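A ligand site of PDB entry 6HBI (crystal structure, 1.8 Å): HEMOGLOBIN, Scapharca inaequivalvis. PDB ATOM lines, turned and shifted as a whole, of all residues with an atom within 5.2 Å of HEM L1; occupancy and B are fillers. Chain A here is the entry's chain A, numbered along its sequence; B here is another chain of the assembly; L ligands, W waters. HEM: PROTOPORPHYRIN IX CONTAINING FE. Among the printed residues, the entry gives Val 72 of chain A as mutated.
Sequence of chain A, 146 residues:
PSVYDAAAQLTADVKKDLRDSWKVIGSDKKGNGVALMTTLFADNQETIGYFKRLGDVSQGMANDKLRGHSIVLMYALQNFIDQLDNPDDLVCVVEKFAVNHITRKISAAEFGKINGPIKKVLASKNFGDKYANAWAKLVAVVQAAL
Thr 47 touches HEM L1 (CG2 to CBC, 3.8 Å). Tyr 50 touches HEM L1. Phe 51 touches HEM L1. Leu 54 touches HEM L1 (CD1 to CGD, 3.6 Å). His 69 touches HEM L1. Val 72 touches HEM L1 (CG1 to CMA, 3.8 Å). Leu 73 touches HEM L1 (CG to C2B, 3.8 Å). Ala 76 touches HEM L1. Leu 77 touches HEM L1. Phe 97 touches HEM L1 (CE1 to CHB, 3.3 Å). Ile 106 touches HEM L1. Glu 110 touches HEM L1. Phe 111 touches HEM L1 (CE1 to CHC, 3.6 Å). Ile 114 touches HEM L1. Hydrophobic or aromatic side chains that line HEM L1: Tyr 50, Phe 51, Leu 54, His 69, Val 72, Leu 73, Ala 76, Leu 77, Phe 97, His 101, Ile 106, Phe 111 and Ile 114. The nearest printed residue that does not touch HEM L1 is Leu 40 (4.3 Å).
The side-chain amide nitrogen (ND2) of Asn 100 of chain A lies within hydrogen-bond range of an oxygen (O2A) of HEM L1, at 3.2 Å. FE of HEM L1 is bound by NE2 of His 101 (2.3 Å). NH2 of Arg 104 is in salt-bridge range of O1A of HEM L1 (2.7 Å). The side-chain amino group (NZ) of Lys 96 of chain B lies within salt-bridge range of an oxygen (O2D) of HEM L1 (2.8 Å). The guanidinium group (NH2) of Arg 53 lies within salt-bridge range of an oxygen (O2D) of HEM L1 (2.9 Å). The side-chain amide nitrogen (ND2) of Asn 100 of chain B is in hydrogen-bond range of an oxygen (O1A) of HEM L1 (3.0 Å). ND2 of Asn 100 of chain A sits at hydrogen-bond distance from O1A of HEM L2, 2.9 Å away. O1A of HEM L2 is in hydrogen-bond range of ND2 of Asn 100 of chain B (3.3 Å).
Water W4 bridges the backbone carbonyl oxygen of Phe 97 and an oxygen (O2A) of HEM L1. Water W5 bridges an oxygen (O1A) of HEM L1 (2.9 Å) and the side-chain amino group (NZ) of Lys 96 of chain B (3.1 Å). Water W3 lies within hydrogen-bond range of the backbone carbonyl oxygen (O) of Tyr 50 (2.8 Å), the backbone NH (N) of Arg 53 (3.0 Å) and an oxygen (O1D) of HEM L1 (3.1 Å).
ND1 of His 69 lies within hydrogen-bond range of NZ of Lys 96 of chain B, at 2.9 Å. ND2 of Asn 100 of chain B sits close to ND2 of Asn 100 of chain A (3.1 Å). The side-chain carboxylate of Glu 110 sits at hydrogen-bond distance from the side-chain hydroxyl of Tyr 50 (3.3 Å). A ring nitrogen (ND1) of His 101 sits at hydrogen-bond distance from the backbone carbonyl oxygen of Phe 97. The backbone carbonyl oxygen of His 101 lies within hydrogen-bond range of the backbone NH of Ile 106 (3.2 Å).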
ATOM      1  N   LEU A  40     -12.013   1.874  10.572  1.00  0.00           N
ATOM      2  CA  LEU A  40     -13.131   2.653  10.070  1.00  0.00           C
ATOM      3  C   LEU A  40     -13.808   3.362  11.230  1.00  0.00           C
ATOM      4  O   LEU A  40     -13.987   4.574  11.214  1.00  0.00           O
ATOM      5  CB  LEU A  40     -14.169   1.767   9.378  1.00  0.00           C
ATOM      6  CG  LEU A  40     -15.402   2.467   8.811  1.00  0.00           C
ATOM      7  CD1 LEU A  40     -15.008   3.447   7.720  1.00  0.00           C
ATOM      8  CD2 LEU A  40     -16.340   1.429   8.251  1.00  0.00           C
ATOM      9  N   THR A  47     -19.678   6.711  11.336  1.00  0.00           N
ATOM     10  CA  THR A  47     -20.259   5.535  10.708  1.00  0.00           C
ATOM     11  C   THR A  47     -20.756   4.494  11.705  1.00  0.00           C
ATOM     12  O   THR A  47     -21.516   3.600  11.317  1.00  0.00           O
ATOM     13  CB  THR A  47     -19.232   4.883   9.750  1.00  0.00           C
ATOM     14  OG1 THR A  47     -18.040   4.606  10.471  1.00  0.00           O
ATOM     15  CG2 THR A  47     -18.918   5.808   8.574  1.00  0.00           C
ATOM     16  N   TYR A  50     -24.525   3.345  11.794  1.00  0.00           N
ATOM     17  CA  TYR A  50     -25.049   2.349  10.861  1.00  0.00           C
ATOM     18  C   TYR A  50     -24.929   0.950  11.433  1.00  0.00           C
ATOM     19  O   TYR A  50     -25.653   0.028  11.053  1.00  0.00           O
ATOM     20  CB  TYR A  50     -24.291   2.357   9.543  1.00  0.00           C
ATOM     21  CG  TYR A  50     -24.544   3.576   8.690  1.00  0.00           C
ATOM     22  CD1 TYR A  50     -25.764   3.715   8.036  1.00  0.00           C
ATOM     23  CD2 TYR A  50     -23.533   4.518   8.503  1.00  0.00           C
ATOM     24  CE1 TYR A  50     -25.986   4.801   7.188  1.00  0.00           C
ATOM     25  CE2 TYR A  50     -23.743   5.609   7.667  1.00  0.00           C
ATOM     26  CZ  TYR A  50     -24.965   5.745   6.999  1.00  0.00           C
ATOM     27  OH  TYR A  50     -25.157   6.793   6.119  1.00  0.00           O
ATOM     28  N   PHE A  51     -24.001   0.769  12.351  1.00  0.00           N
ATOM     29  CA  PHE A  51     -23.716  -0.534  12.888  1.00  0.00           C
ATOM     30  C   PHE A  51     -24.243  -0.719  14.308  1.00  0.00           C
ATOM     31  O   PHE A  51     -23.659  -1.452  15.113  1.00  0.00           O
ATOM     32  CB  PHE A  51     -22.219  -0.740  12.813  1.00  0.00           C
ATOM     33  CG  PHE A  51     -21.672  -0.829  11.398  1.00  0.00           C
ATOM     34  CD1 PHE A  51     -21.581  -2.061  10.747  1.00  0.00           C
ATOM     35  CD2 PHE A  51     -21.194   0.329  10.758  1.00  0.00           C
ATOM     36  CE1 PHE A  51     -21.029  -2.134   9.475  1.00  0.00           C
ATOM     37  CE2 PHE A  51     -20.639   0.242   9.488  1.00  0.00           C
ATOM     38  CZ  PHE A  51     -20.548  -0.981   8.843  1.00  0.00           C
ATOM     39  N   ARG A  53     -26.568  -2.533  15.385  1.00  0.00           N
ATOM     40  CA  ARG A  53     -26.830  -3.936  15.688  1.00  0.00           C
ATOM     41  C   ARG A  53     -25.592  -4.658  16.216  1.00  0.00           C
ATOM     42  O   ARG A  53     -25.703  -5.609  16.989  1.00  0.00           O
ATOM     43  CB  ARG A  53     -27.336  -4.644  14.432  1.00  0.00           C
ATOM     44  CG  ARG A  53     -28.011  -5.971  14.732  1.00  0.00           C
ATOM     45  CD  ARG A  53     -28.209  -6.813  13.474  1.00  0.00           C
ATOM     46  NE  ARG A  53     -26.940  -7.256  12.905  1.00  0.00           N
ATOM     47  CZ  ARG A  53     -26.276  -8.315  13.350  1.00  0.00           C
ATOM     48  NH1 ARG A  53     -26.721  -9.049  14.367  1.00  0.00           N
ATOM     49  NH2 ARG A  53     -25.139  -8.646  12.767  1.00  0.00           N
ATOM     50  N   LEU A  54     -24.381  -4.218  15.839  1.00  0.00           N
ATOM     51  CA  LEU A  54     -23.148  -4.851  16.301  1.00  0.00           C
ATOM     52  C   LEU A  54     -22.870  -4.609  17.781  1.00  0.00           C
ATOM     53  O   LEU A  54     -22.115  -5.358  18.394  1.00  0.00           O
ATOM     54  CB  LEU A  54     -21.988  -4.335  15.464  1.00  0.00           C
ATOM     55  CG  LEU A  54     -21.675  -5.078  14.158  1.00  0.00           C
ATOM     56  CD1 LEU A  54     -22.898  -5.213  13.284  1.00  0.00           C
ATOM     57  CD2 LEU A  54     -20.628  -4.299  13.408  1.00  0.00           C
ATOM     58  N   HIS A  69     -19.354 -10.163  11.233  1.00  0.00           N
ATOM     59  CA  HIS A  69     -19.452  -9.202  10.138  1.00  0.00           C
ATOM     60  C   HIS A  69     -18.136  -9.062   9.397  1.00  0.00           C
ATOM     61  O   HIS A  69     -18.123  -9.116   8.171  1.00  0.00           O
ATOM     62  CB  HIS A  69     -19.888  -7.810  10.673  1.00  0.00           C
ATOM     63  CG  HIS A  69     -19.845  -6.679   9.631  1.00  0.00           C
ATOM     64  ND1 HIS A  69     -20.790  -6.595   8.718  1.00  0.00           N
ATOM     65  CD2 HIS A  69     -18.827  -5.777   9.453  1.00  0.00           C
ATOM     66  CE1 HIS A  69     -20.363  -5.622   7.940  1.00  0.00           C
ATOM     67  NE2 HIS A  69     -19.215  -5.147   8.368  1.00  0.00           N
ATOM     68  N   VAL A  72     -17.352 -12.086   7.185  1.00  0.00           N
ATOM     69  CA  VAL A  72     -18.217 -12.066   6.002  1.00  0.00           C
ATOM     70  C   VAL A  72     -17.799 -10.972   5.012  1.00  0.00           C
ATOM     71  O   VAL A  72     -17.741 -11.192   3.789  1.00  0.00           O
ATOM     72  CB  VAL A  72     -19.688 -11.907   6.489  1.00  0.00           C
ATOM     73  CG1 VAL A  72     -20.666 -11.612   5.352  1.00  0.00           C
ATOM     74  CG2 VAL A  72     -20.122 -13.230   7.073  1.00  0.00           C
ATOM     75  N   LEU A  73     -17.419  -9.796   5.503  1.00  0.00           N
ATOM     76  CA  LEU A  73     -16.952  -8.715   4.648  1.00  0.00           C
ATOM     77  C   LEU A  73     -15.741  -9.173   3.819  1.00  0.00           C
ATOM     78  O   LEU A  73     -15.665  -8.939   2.608  1.00  0.00           O
ATOM     79  CB  LEU A  73     -16.602  -7.505   5.534  1.00  0.00           C
ATOM     80  CG  LEU A  73     -16.047  -6.189   4.984  1.00  0.00           C
ATOM     81  CD1 LEU A  73     -16.379  -5.097   5.980  1.00  0.00           C
ATOM     82  CD2 LEU A  73     -14.537  -6.246   4.767  1.00  0.00           C
ATOM     83  N   ALA A  76     -16.668 -11.168   0.691  1.00  0.00           N
ATOM     84  CA  ALA A  76     -17.150 -10.323  -0.402  1.00  0.00           C
ATOM     85  C   ALA A  76     -15.964  -9.802  -1.208  1.00  0.00           C
ATOM     86  O   ALA A  76     -15.976  -9.767  -2.445  1.00  0.00           O
ATOM     87  CB  ALA A  76     -17.911  -9.110   0.126  1.00  0.00           C
ATOM     88  N   LEU A  77     -14.891  -9.374  -0.521  1.00  0.00           N
ATOM     89  CA  LEU A  77     -13.679  -8.958  -1.217  1.00  0.00           C
ATOM     90  C   LEU A  77     -13.053 -10.120  -1.978  1.00  0.00           C
ATOM     91  O   LEU A  77     -12.680  -9.938  -3.136  1.00  0.00           O
ATOM     92  CB  LEU A  77     -12.692  -8.387  -0.234  1.00  0.00           C
ATOM     93  CG  LEU A  77     -12.641  -6.879   0.039  1.00  0.00           C
ATOM     94  CD1 LEU A  77     -13.793  -6.121  -0.600  1.00  0.00           C
ATOM     95  CD2 LEU A  77     -12.631  -6.731   1.548  1.00  0.00           C
ATOM     96  N   PHE A  80     -14.888 -10.472  -5.116  1.00  0.00           N
ATOM     97  CA  PHE A  80     -14.532  -9.482  -6.130  1.00  0.00           C
ATOM     98  C   PHE A  80     -13.204  -9.825  -6.800  1.00  0.00           C
ATOM     99  O   PHE A  80     -13.122  -9.785  -8.024  1.00  0.00           O
ATOM    100  CB  PHE A  80     -14.423  -8.071  -5.534  1.00  0.00           C
ATOM    101  CG  PHE A  80     -15.731  -7.463  -4.984  1.00  0.00           C
ATOM    102  CD1 PHE A  80     -16.986  -7.858  -5.428  1.00  0.00           C
ATOM    103  CD2 PHE A  80     -15.634  -6.482  -3.986  1.00  0.00           C
ATOM    104  CE1 PHE A  80     -18.143  -7.295  -4.876  1.00  0.00           C
ATOM    105  CE2 PHE A  80     -16.793  -5.914  -3.443  1.00  0.00           C
ATOM    106  CZ  PHE A  80     -18.046  -6.323  -3.884  1.00  0.00           C
ATOM    107  N   PHE A  97     -24.306  -7.175  -4.665  1.00  0.00           N
ATOM    108  CA  PHE A  97     -23.740  -6.677  -3.412  1.00  0.00           C
ATOM    109  C   PHE A  97     -24.304  -5.325  -2.987  1.00  0.00           C
ATOM    110  O   PHE A  97     -24.501  -5.032  -1.788  1.00  0.00           O
ATOM    111  CB  PHE A  97     -22.236  -6.584  -3.605  1.00  0.00           C
ATOM    112  CG  PHE A  97     -21.471  -5.929  -2.481  1.00  0.00           C
ATOM    113  CD1 PHE A  97     -21.062  -6.701  -1.394  1.00  0.00           C
ATOM    114  CD2 PHE A  97     -21.148  -4.579  -2.568  1.00  0.00           C
ATOM    115  CE1 PHE A  97     -20.321  -6.096  -0.380  1.00  0.00           C
ATOM    116  CE2 PHE A  97     -20.405  -3.979  -1.545  1.00  0.00           C
ATOM    117  CZ  PHE A  97     -20.019  -4.732  -0.452  1.00  0.00           C
ATOM    118  N   ASN A 100     -28.237  -4.445  -0.722  1.00  0.00           N
ATOM    119  CA  ASN A 100     -28.407  -4.174   0.699  1.00  0.00           C
ATOM    120  C   ASN A 100     -27.776  -2.863   1.154  1.00  0.00           C
ATOM    121  O   ASN A 100     -28.296  -2.221   2.069  1.00  0.00           O
ATOM    122  CB  ASN A 100     -27.852  -5.320   1.522  1.00  0.00           C
ATOM    123  CG  ASN A 100     -28.662  -6.597   1.382  1.00  0.00           C
ATOM    124  OD1 ASN A 100     -29.806  -6.603   0.906  1.00  0.00           O
ATOM    125  ND2 ASN A 100     -28.131  -7.744   1.775  1.00  0.00           N
ATOM    126  N   HIS A 101     -26.720  -2.371   0.502  1.00  0.00           N
ATOM    127  CA  HIS A 101     -26.119  -1.119   0.917  1.00  0.00           C
ATOM    128  C   HIS A 101     -27.029   0.030   0.489  1.00  0.00           C
ATOM    129  O   HIS A 101     -27.223   0.979   1.247  1.00  0.00           O
ATOM    130  CB  HIS A 101     -24.708  -0.981   0.293  1.00  0.00           C
ATOM    131  CG  HIS A 101     -23.752  -1.984   0.957  1.00  0.00           C
ATOM    132  ND1 HIS A 101     -23.554  -3.317   0.565  1.00  0.00           N
ATOM    133  CD2 HIS A 101     -22.992  -1.694   2.097  1.00  0.00           C
ATOM    134  CE1 HIS A 101     -22.719  -3.821   1.503  1.00  0.00           C
ATOM    135  NE2 HIS A 101     -22.366  -2.918   2.390  1.00  0.00           N
ATOM    136  N   ARG A 104     -29.807   0.406   2.860  1.00  0.00           N
ATOM    137  CA  ARG A 104     -29.344   1.068   4.075  1.00  0.00           C
ATOM    138  C   ARG A 104     -28.986   2.532   3.940  1.00  0.00           C
ATOM    139  O   ARG A 104     -28.538   3.166   4.899  1.00  0.00           O
ATOM    140  CB  ARG A 104     -28.125   0.352   4.612  1.00  0.00           C
ATOM    141  CG  ARG A 104     -28.442  -1.005   5.141  1.00  0.00           C
ATOM    142  CD  ARG A 104     -27.132  -1.695   5.377  1.00  0.00           C
ATOM    143  NE  ARG A 104     -27.498  -3.066   5.645  1.00  0.00           N
ATOM    144  CZ  ARG A 104     -26.961  -4.094   5.005  1.00  0.00           C
ATOM    145  NH1 ARG A 104     -25.991  -3.966   4.066  1.00  0.00           N
ATOM    146  NH2 ARG A 104     -27.504  -5.272   5.300  1.00  0.00           N
ATOM    147  N   ILE A 106     -26.568   3.963   2.219  1.00  0.00           N
ATOM    148  CA  ILE A 106     -25.137   4.127   2.286  1.00  0.00           C
ATOM    149  C   ILE A 106     -24.897   4.708   0.905  1.00  0.00           C
ATOM    150  O   ILE A 106     -25.181   4.069  -0.117  1.00  0.00           O
ATOM    151  CB  ILE A 106     -24.334   2.794   2.400  1.00  0.00           C
ATOM    152  CG1 ILE A 106     -24.836   1.846   3.493  1.00  0.00           C
ATOM    153  CG2 ILE A 106     -22.892   3.176   2.684  1.00  0.00           C
ATOM    154  CD1 ILE A 106     -24.696   2.301   4.951  1.00  0.00           C
ATOM    155  N   GLU A 110     -20.244   7.746   1.354  1.00  0.00           N
ATOM    156  CA  GLU A 110     -20.109   7.077   2.645  1.00  0.00           C
ATOM    157  C   GLU A 110     -19.320   5.775   2.503  1.00  0.00           C
ATOM    158  O   GLU A 110     -18.496   5.434   3.351  1.00  0.00           O
ATOM    159  CB  GLU A 110     -21.478   6.762   3.194  1.00  0.00           C
ATOM    160  CG  GLU A 110     -21.544   6.480   4.688  1.00  0.00           C
ATOM    161  CD  GLU A 110     -21.772   7.700   5.577  1.00  0.00           C
ATOM    162  OE1 GLU A 110     -22.550   8.584   5.201  1.00  0.00           O
ATOM    163  OE2 GLU A 110     -21.205   7.751   6.659  1.00  0.00           O
ATOM    164  N   PHE A 111     -19.571   5.034   1.420  1.00  0.00           N
ATOM    165  CA  PHE A 111     -18.859   3.793   1.143  1.00  0.00           C
ATOM    166  C   PHE A 111     -17.374   4.062   0.932  1.00  0.00           C
ATOM    167  O   PHE A 111     -16.506   3.316   1.393  1.00  0.00           O
ATOM    168  CB  PHE A 111     -19.441   3.133  -0.098  1.00  0.00           C
ATOM    169  CG  PHE A 111     -19.069   1.662  -0.286  1.00  0.00           C
ATOM    170  CD1 PHE A 111     -19.845   0.670   0.325  1.00  0.00           C
ATOM    171  CD2 PHE A 111     -17.965   1.299  -1.061  1.00  0.00           C
ATOM    172  CE1 PHE A 111     -19.497  -0.674   0.162  1.00  0.00           C
ATOM    173  CE2 PHE A 111     -17.637  -0.048  -1.221  1.00  0.00           C
ATOM    174  CZ  PHE A 111     -18.403  -1.039  -0.612  1.00  0.00           C
ATOM    175  N   ILE A 114     -14.202   3.663   3.411  1.00  0.00           N
ATOM    176  CA  ILE A 114     -13.393   2.475   3.613  1.00  0.00           C
ATOM    177  C   ILE A 114     -11.989   2.607   2.999  1.00  0.00           C
ATOM    178  O   ILE A 114     -11.073   1.878   3.397  1.00  0.00           O
ATOM    179  CB  ILE A 114     -14.176   1.247   3.022  1.00  0.00           C
ATOM    180  CG1 ILE A 114     -13.653  -0.018   3.696  1.00  0.00           C
ATOM    181  CG2 ILE A 114     -14.032   1.161   1.495  1.00  0.00           C
ATOM    182  CD1 ILE A 114     -14.097  -0.131   5.173  1.00  0.00           C
ATOM    183  N   ILE A 118      -8.454   0.678   4.259  1.00  0.00           N
ATOM    184  CA  ILE A 118      -7.761  -0.233   3.345  1.00  0.00           C
ATOM    185  C   ILE A 118      -6.302   0.221   3.196  1.00  0.00           C
ATOM    186  O   ILE A 118      -5.395  -0.599   3.382  1.00  0.00           O
ATOM    187  CB  ILE A 118      -8.482  -0.265   1.967  1.00  0.00           C
ATOM    188  CG1 ILE A 118      -9.827  -0.963   2.149  1.00  0.00           C
ATOM    189  CG2 ILE A 118      -7.656  -1.004   0.915  1.00  0.00           C
ATOM    190  CD1 ILE A 118     -10.682  -1.081   0.864  1.00  0.00           C
ATOM    191  N   VAL A 139     -12.977  -0.157  -5.229  1.00  0.00           N
ATOM    192  CA  VAL A 139     -14.045   0.434  -4.419  1.00  0.00           C
ATOM    193  C   VAL A 139     -14.917   1.373  -5.280  1.00  0.00           C
ATOM    194  O   VAL A 139     -16.147   1.421  -5.114  1.00  0.00           O
ATOM    195  CB  VAL A 139     -13.410   1.185  -3.209  1.00  0.00           C
ATOM    196  CG1 VAL A 139     -14.440   1.947  -2.388  1.00  0.00           C
ATOM    197  CG2 VAL A 139     -12.778   0.150  -2.278  1.00  0.00           C
ATOM    198  N   LYS B  96     -24.569 -14.124  11.741  1.00  0.00           N
ATOM    199  CA  LYS B  96     -24.490 -12.944  10.866  1.00  0.00           C
ATOM    200  C   LYS B  96     -25.270 -13.207   9.590  1.00  0.00           C
ATOM    201  O   LYS B  96     -26.123 -12.408   9.195  1.00  0.00           O
ATOM    202  CB  LYS B  96     -23.027 -12.609  10.495  1.00  0.00           C
ATOM    203  CG  LYS B  96     -22.748 -11.628   9.341  1.00  0.00           C
ATOM    204  CD  LYS B  96     -23.234 -10.201   9.596  1.00  0.00           C
ATOM    205  CE  LYS B  96     -22.974  -9.386   8.331  1.00  0.00           C
ATOM    206  NZ  LYS B  96     -23.312  -7.985   8.479  1.00  0.00           N
ATOM    207  N   ASN B 100     -30.303 -11.379   7.655  1.00  0.00           N
ATOM    208  CA  ASN B 100     -31.149 -10.966   6.542  1.00  0.00           C
ATOM    209  C   ASN B 100     -32.189 -12.002   6.145  1.00  0.00           C
ATOM    210  O   ASN B 100     -33.299 -11.667   5.728  1.00  0.00           O
ATOM    211  CB  ASN B 100     -30.307 -10.645   5.310  1.00  0.00           C
ATOM    212  CG  ASN B 100     -29.483  -9.367   5.410  1.00  0.00           C
ATOM    213  OD1 ASN B 100     -29.666  -8.497   6.274  1.00  0.00           O
ATOM    214  ND2 ASN B 100     -28.547  -9.179   4.505  1.00  0.00           N
HETATM  215  CHA HEM L   1     -23.237  -5.474   5.644  1.00  0.00           C
HETATM  216  CHB HEM L   1     -19.445  -5.903   2.791  1.00  0.00           C
HETATM  217  CHC HEM L   1     -18.385  -1.313   3.497  1.00  0.00           C
HETATM  218  CHD HEM L   1     -22.426  -0.768   6.009  1.00  0.00           C
HETATM  219  C1A HEM L   1     -22.360  -5.988   4.706  1.00  0.00           C
HETATM  220  C2A HEM L   1     -22.277  -7.380   4.310  1.00  0.00           C
HETATM  221  C3A HEM L   1     -21.205  -7.490   3.507  1.00  0.00           C
HETATM  222  C4A HEM L   1     -20.618  -6.177   3.431  1.00  0.00           C
HETATM  223  CMA HEM L   1     -20.717  -8.754   2.808  1.00  0.00           C
HETATM  224  CAA HEM L   1     -23.203  -8.535   4.668  1.00  0.00           C
HETATM  225  CBA HEM L   1     -24.329  -8.740   3.663  1.00  0.00           C
HETATM  226  CGA HEM L   1     -25.313  -7.573   3.656  1.00  0.00           C
HETATM  227  O1A HEM L   1     -26.105  -7.506   4.593  1.00  0.00           O
HETATM  228  O2A HEM L   1     -25.293  -6.741   2.750  1.00  0.00           O
HETATM  229  C1B HEM L   1     -18.847  -4.677   2.704  1.00  0.00           C
HETATM  230  C2B HEM L   1     -17.591  -4.462   2.028  1.00  0.00           C
HETATM  231  C3B HEM L   1     -17.248  -3.172   2.262  1.00  0.00           C
HETATM  232  C4B HEM L   1     -18.349  -2.609   3.040  1.00  0.00           C
HETATM  233  CMB HEM L   1     -16.857  -5.528   1.211  1.00  0.00           C
HETATM  234  CAB HEM L   1     -16.063  -2.522   1.963  1.00  0.00           C
HETATM  235  CBB HEM L   1     -15.334  -2.579   0.710  1.00  0.00           C
HETATM  236  C1C HEM L   1     -19.415  -0.757   4.214  1.00  0.00           C
HETATM  237  C2C HEM L   1     -19.435   0.620   4.655  1.00  0.00           C
HETATM  238  C3C HEM L   1     -20.616   0.808   5.331  1.00  0.00           C
HETATM  239  C4C HEM L   1     -21.282  -0.480   5.289  1.00  0.00           C
HETATM  240  CMC HEM L   1     -18.298   1.603   4.408  1.00  0.00           C
HETATM  241  CAC HEM L   1     -21.185   1.945   5.890  1.00  0.00           C
HETATM  242  CBC HEM L   1     -20.503   3.080   6.476  1.00  0.00           C
HETATM  243  C1D HEM L   1     -22.974  -2.019   6.174  1.00  0.00           C
HETATM  244  C2D HEM L   1     -23.952  -2.337   7.191  1.00  0.00           C
HETATM  245  C3D HEM L   1     -24.118  -3.672   7.145  1.00  0.00           C
HETATM  246  C4D HEM L   1     -23.280  -4.171   6.070  1.00  0.00           C
HETATM  247  CMD HEM L   1     -24.612  -1.356   8.164  1.00  0.00           C
HETATM  248  CAD HEM L   1     -24.954  -4.492   8.100  1.00  0.00           C
HETATM  249  CBD HEM L   1     -24.178  -4.857   9.360  1.00  0.00           C
HETATM  250  CGD HEM L   1     -25.024  -5.628  10.348  1.00  0.00           C
HETATM  251  O1D HEM L   1     -25.901  -5.031  10.986  1.00  0.00           O
HETATM  252  O2D HEM L   1     -24.811  -6.828  10.495  1.00  0.00           O
HETATM  253  NA  HEM L   1     -21.358  -5.242   4.119  1.00  0.00           N
HETATM  254  NB  HEM L   1     -19.341  -3.529   3.286  1.00  0.00           N
HETATM  255  NC  HEM L   1     -20.553  -1.428   4.583  1.00  0.00           N
HETATM  256  ND  HEM L   1     -22.528  -3.147   5.522  1.00  0.00           N
HETATM  257 FE   HEM L   1     -21.079  -3.291   4.202  1.00  0.00          FE
HETATM  258  CHA HEM L   2     -29.807 -13.673  -0.222  1.00  0.00           C
HETATM  259  CHB HEM L   2     -26.983 -17.396   0.765  1.00  0.00           C
HETATM  260  CHC HEM L   2     -30.812 -20.247   0.814  1.00  0.00           C
HETATM  261  CHD HEM L   2     -33.696 -16.483   0.077  1.00  0.00           C
HETATM  262  C1A HEM L   2     -28.710 -14.417   0.150  1.00  0.00           C
HETATM  263  C2A HEM L   2     -27.343 -13.926   0.184  1.00  0.00           C
HETATM  264  C3A HEM L   2     -26.561 -14.988   0.449  1.00  0.00           C
HETATM  265  C4A HEM L   2     -27.434 -16.119   0.564  1.00  0.00           C
HETATM  266  CMA HEM L   2     -25.055 -14.998   0.664  1.00  0.00           C
HETATM  267  CAA HEM L   2     -26.875 -12.494   0.010  1.00  0.00           C
HETATM  268  CBA HEM L   2     -26.761 -11.717   1.312  1.00  0.00           C
HETATM  269  CGA HEM L   2     -28.109 -11.462   1.970  1.00  0.00           C
HETATM  270  O1A HEM L   2     -28.779 -10.545   1.546  1.00  0.00           O
HETATM  271  O2A HEM L   2     -28.507 -12.173   2.878  1.00  0.00           O
HETATM  272  C1B HEM L   2     -27.790 -18.496   0.929  1.00  0.00           C
HETATM  273  C2B HEM L   2     -27.263 -19.829   1.109  1.00  0.00           C
HETATM  274  C3B HEM L   2     -28.337 -20.667   1.053  1.00  0.00           C
HETATM  275  C4B HEM L   2     -29.509 -19.799   0.913  1.00  0.00           C
HETATM  276  CMB HEM L   2     -25.786 -20.135   1.379  1.00  0.00           C
HETATM  277  CAB HEM L   2     -28.417 -22.075   1.070  1.00  0.00           C
HETATM  278  CBB HEM L   2     -27.387 -23.063   1.394  1.00  0.00           C
HETATM  279  C1C HEM L   2     -31.950 -19.458   0.688  1.00  0.00           C
HETATM  280  C2C HEM L   2     -33.289 -19.994   0.557  1.00  0.00           C
HETATM  281  C3C HEM L   2     -34.124 -18.927   0.396  1.00  0.00           C
HETATM  282  C4C HEM L   2     -33.269 -17.755   0.421  1.00  0.00           C
HETATM  283  CMC HEM L   2     -33.609 -21.484   0.604  1.00  0.00           C
HETATM  284  CAC HEM L   2     -35.522 -18.874   0.286  1.00  0.00           C
HETATM  285  CBC HEM L   2     -36.397 -19.831  -0.363  1.00  0.00           C
HETATM  286  C1D HEM L   2     -32.879 -15.397  -0.099  1.00  0.00           C
HETATM  287  C2D HEM L   2     -33.318 -14.163  -0.682  1.00  0.00           C
HETATM  288  C3D HEM L   2     -32.209 -13.396  -0.814  1.00  0.00           C
HETATM  289  C4D HEM L   2     -31.109 -14.140  -0.273  1.00  0.00           C
HETATM  290  CMD HEM L   2     -34.740 -13.815  -1.111  1.00  0.00           C
HETATM  291  CAD HEM L   2     -32.113 -12.053  -1.532  1.00  0.00           C
HETATM  292  CBD HEM L   2     -32.075 -12.236  -3.041  1.00  0.00           C
HETATM  293  CGD HEM L   2     -32.175 -10.920  -3.780  1.00  0.00           C
HETATM  294  O1D HEM L   2     -33.287 -10.423  -3.986  1.00  0.00           O
HETATM  295  O2D HEM L   2     -31.129 -10.381  -4.133  1.00  0.00           O
HETATM  296  NA  HEM L   2     -28.764 -15.759   0.456  1.00  0.00           N
HETATM  297  NB  HEM L   2     -29.165 -18.456   0.877  1.00  0.00           N
HETATM  298  NC  HEM L   2     -31.946 -18.073   0.630  1.00  0.00           N
HETATM  299  ND  HEM L   2     -31.507 -15.394   0.127  1.00  0.00           N
HETATM  300 FE   HEM L   2     -30.383 -16.868   0.776  1.00  0.00          FE
HETATM  301  O   HOH W   1     -24.555 -11.268   6.032  1.00  0.00           O
HETATM  302  O   HOH W   2     -18.675  -2.751   6.760  1.00  0.00           O
HETATM  303  O   HOH W   3     -26.385  -2.285  12.428  1.00  0.00           O
HETATM  304  O   HOH W   4     -24.069  -6.815   0.189  1.00  0.00           O
HETATM  305  O   HOH W   5     -26.199  -8.166   7.437  1.00  0.00           O
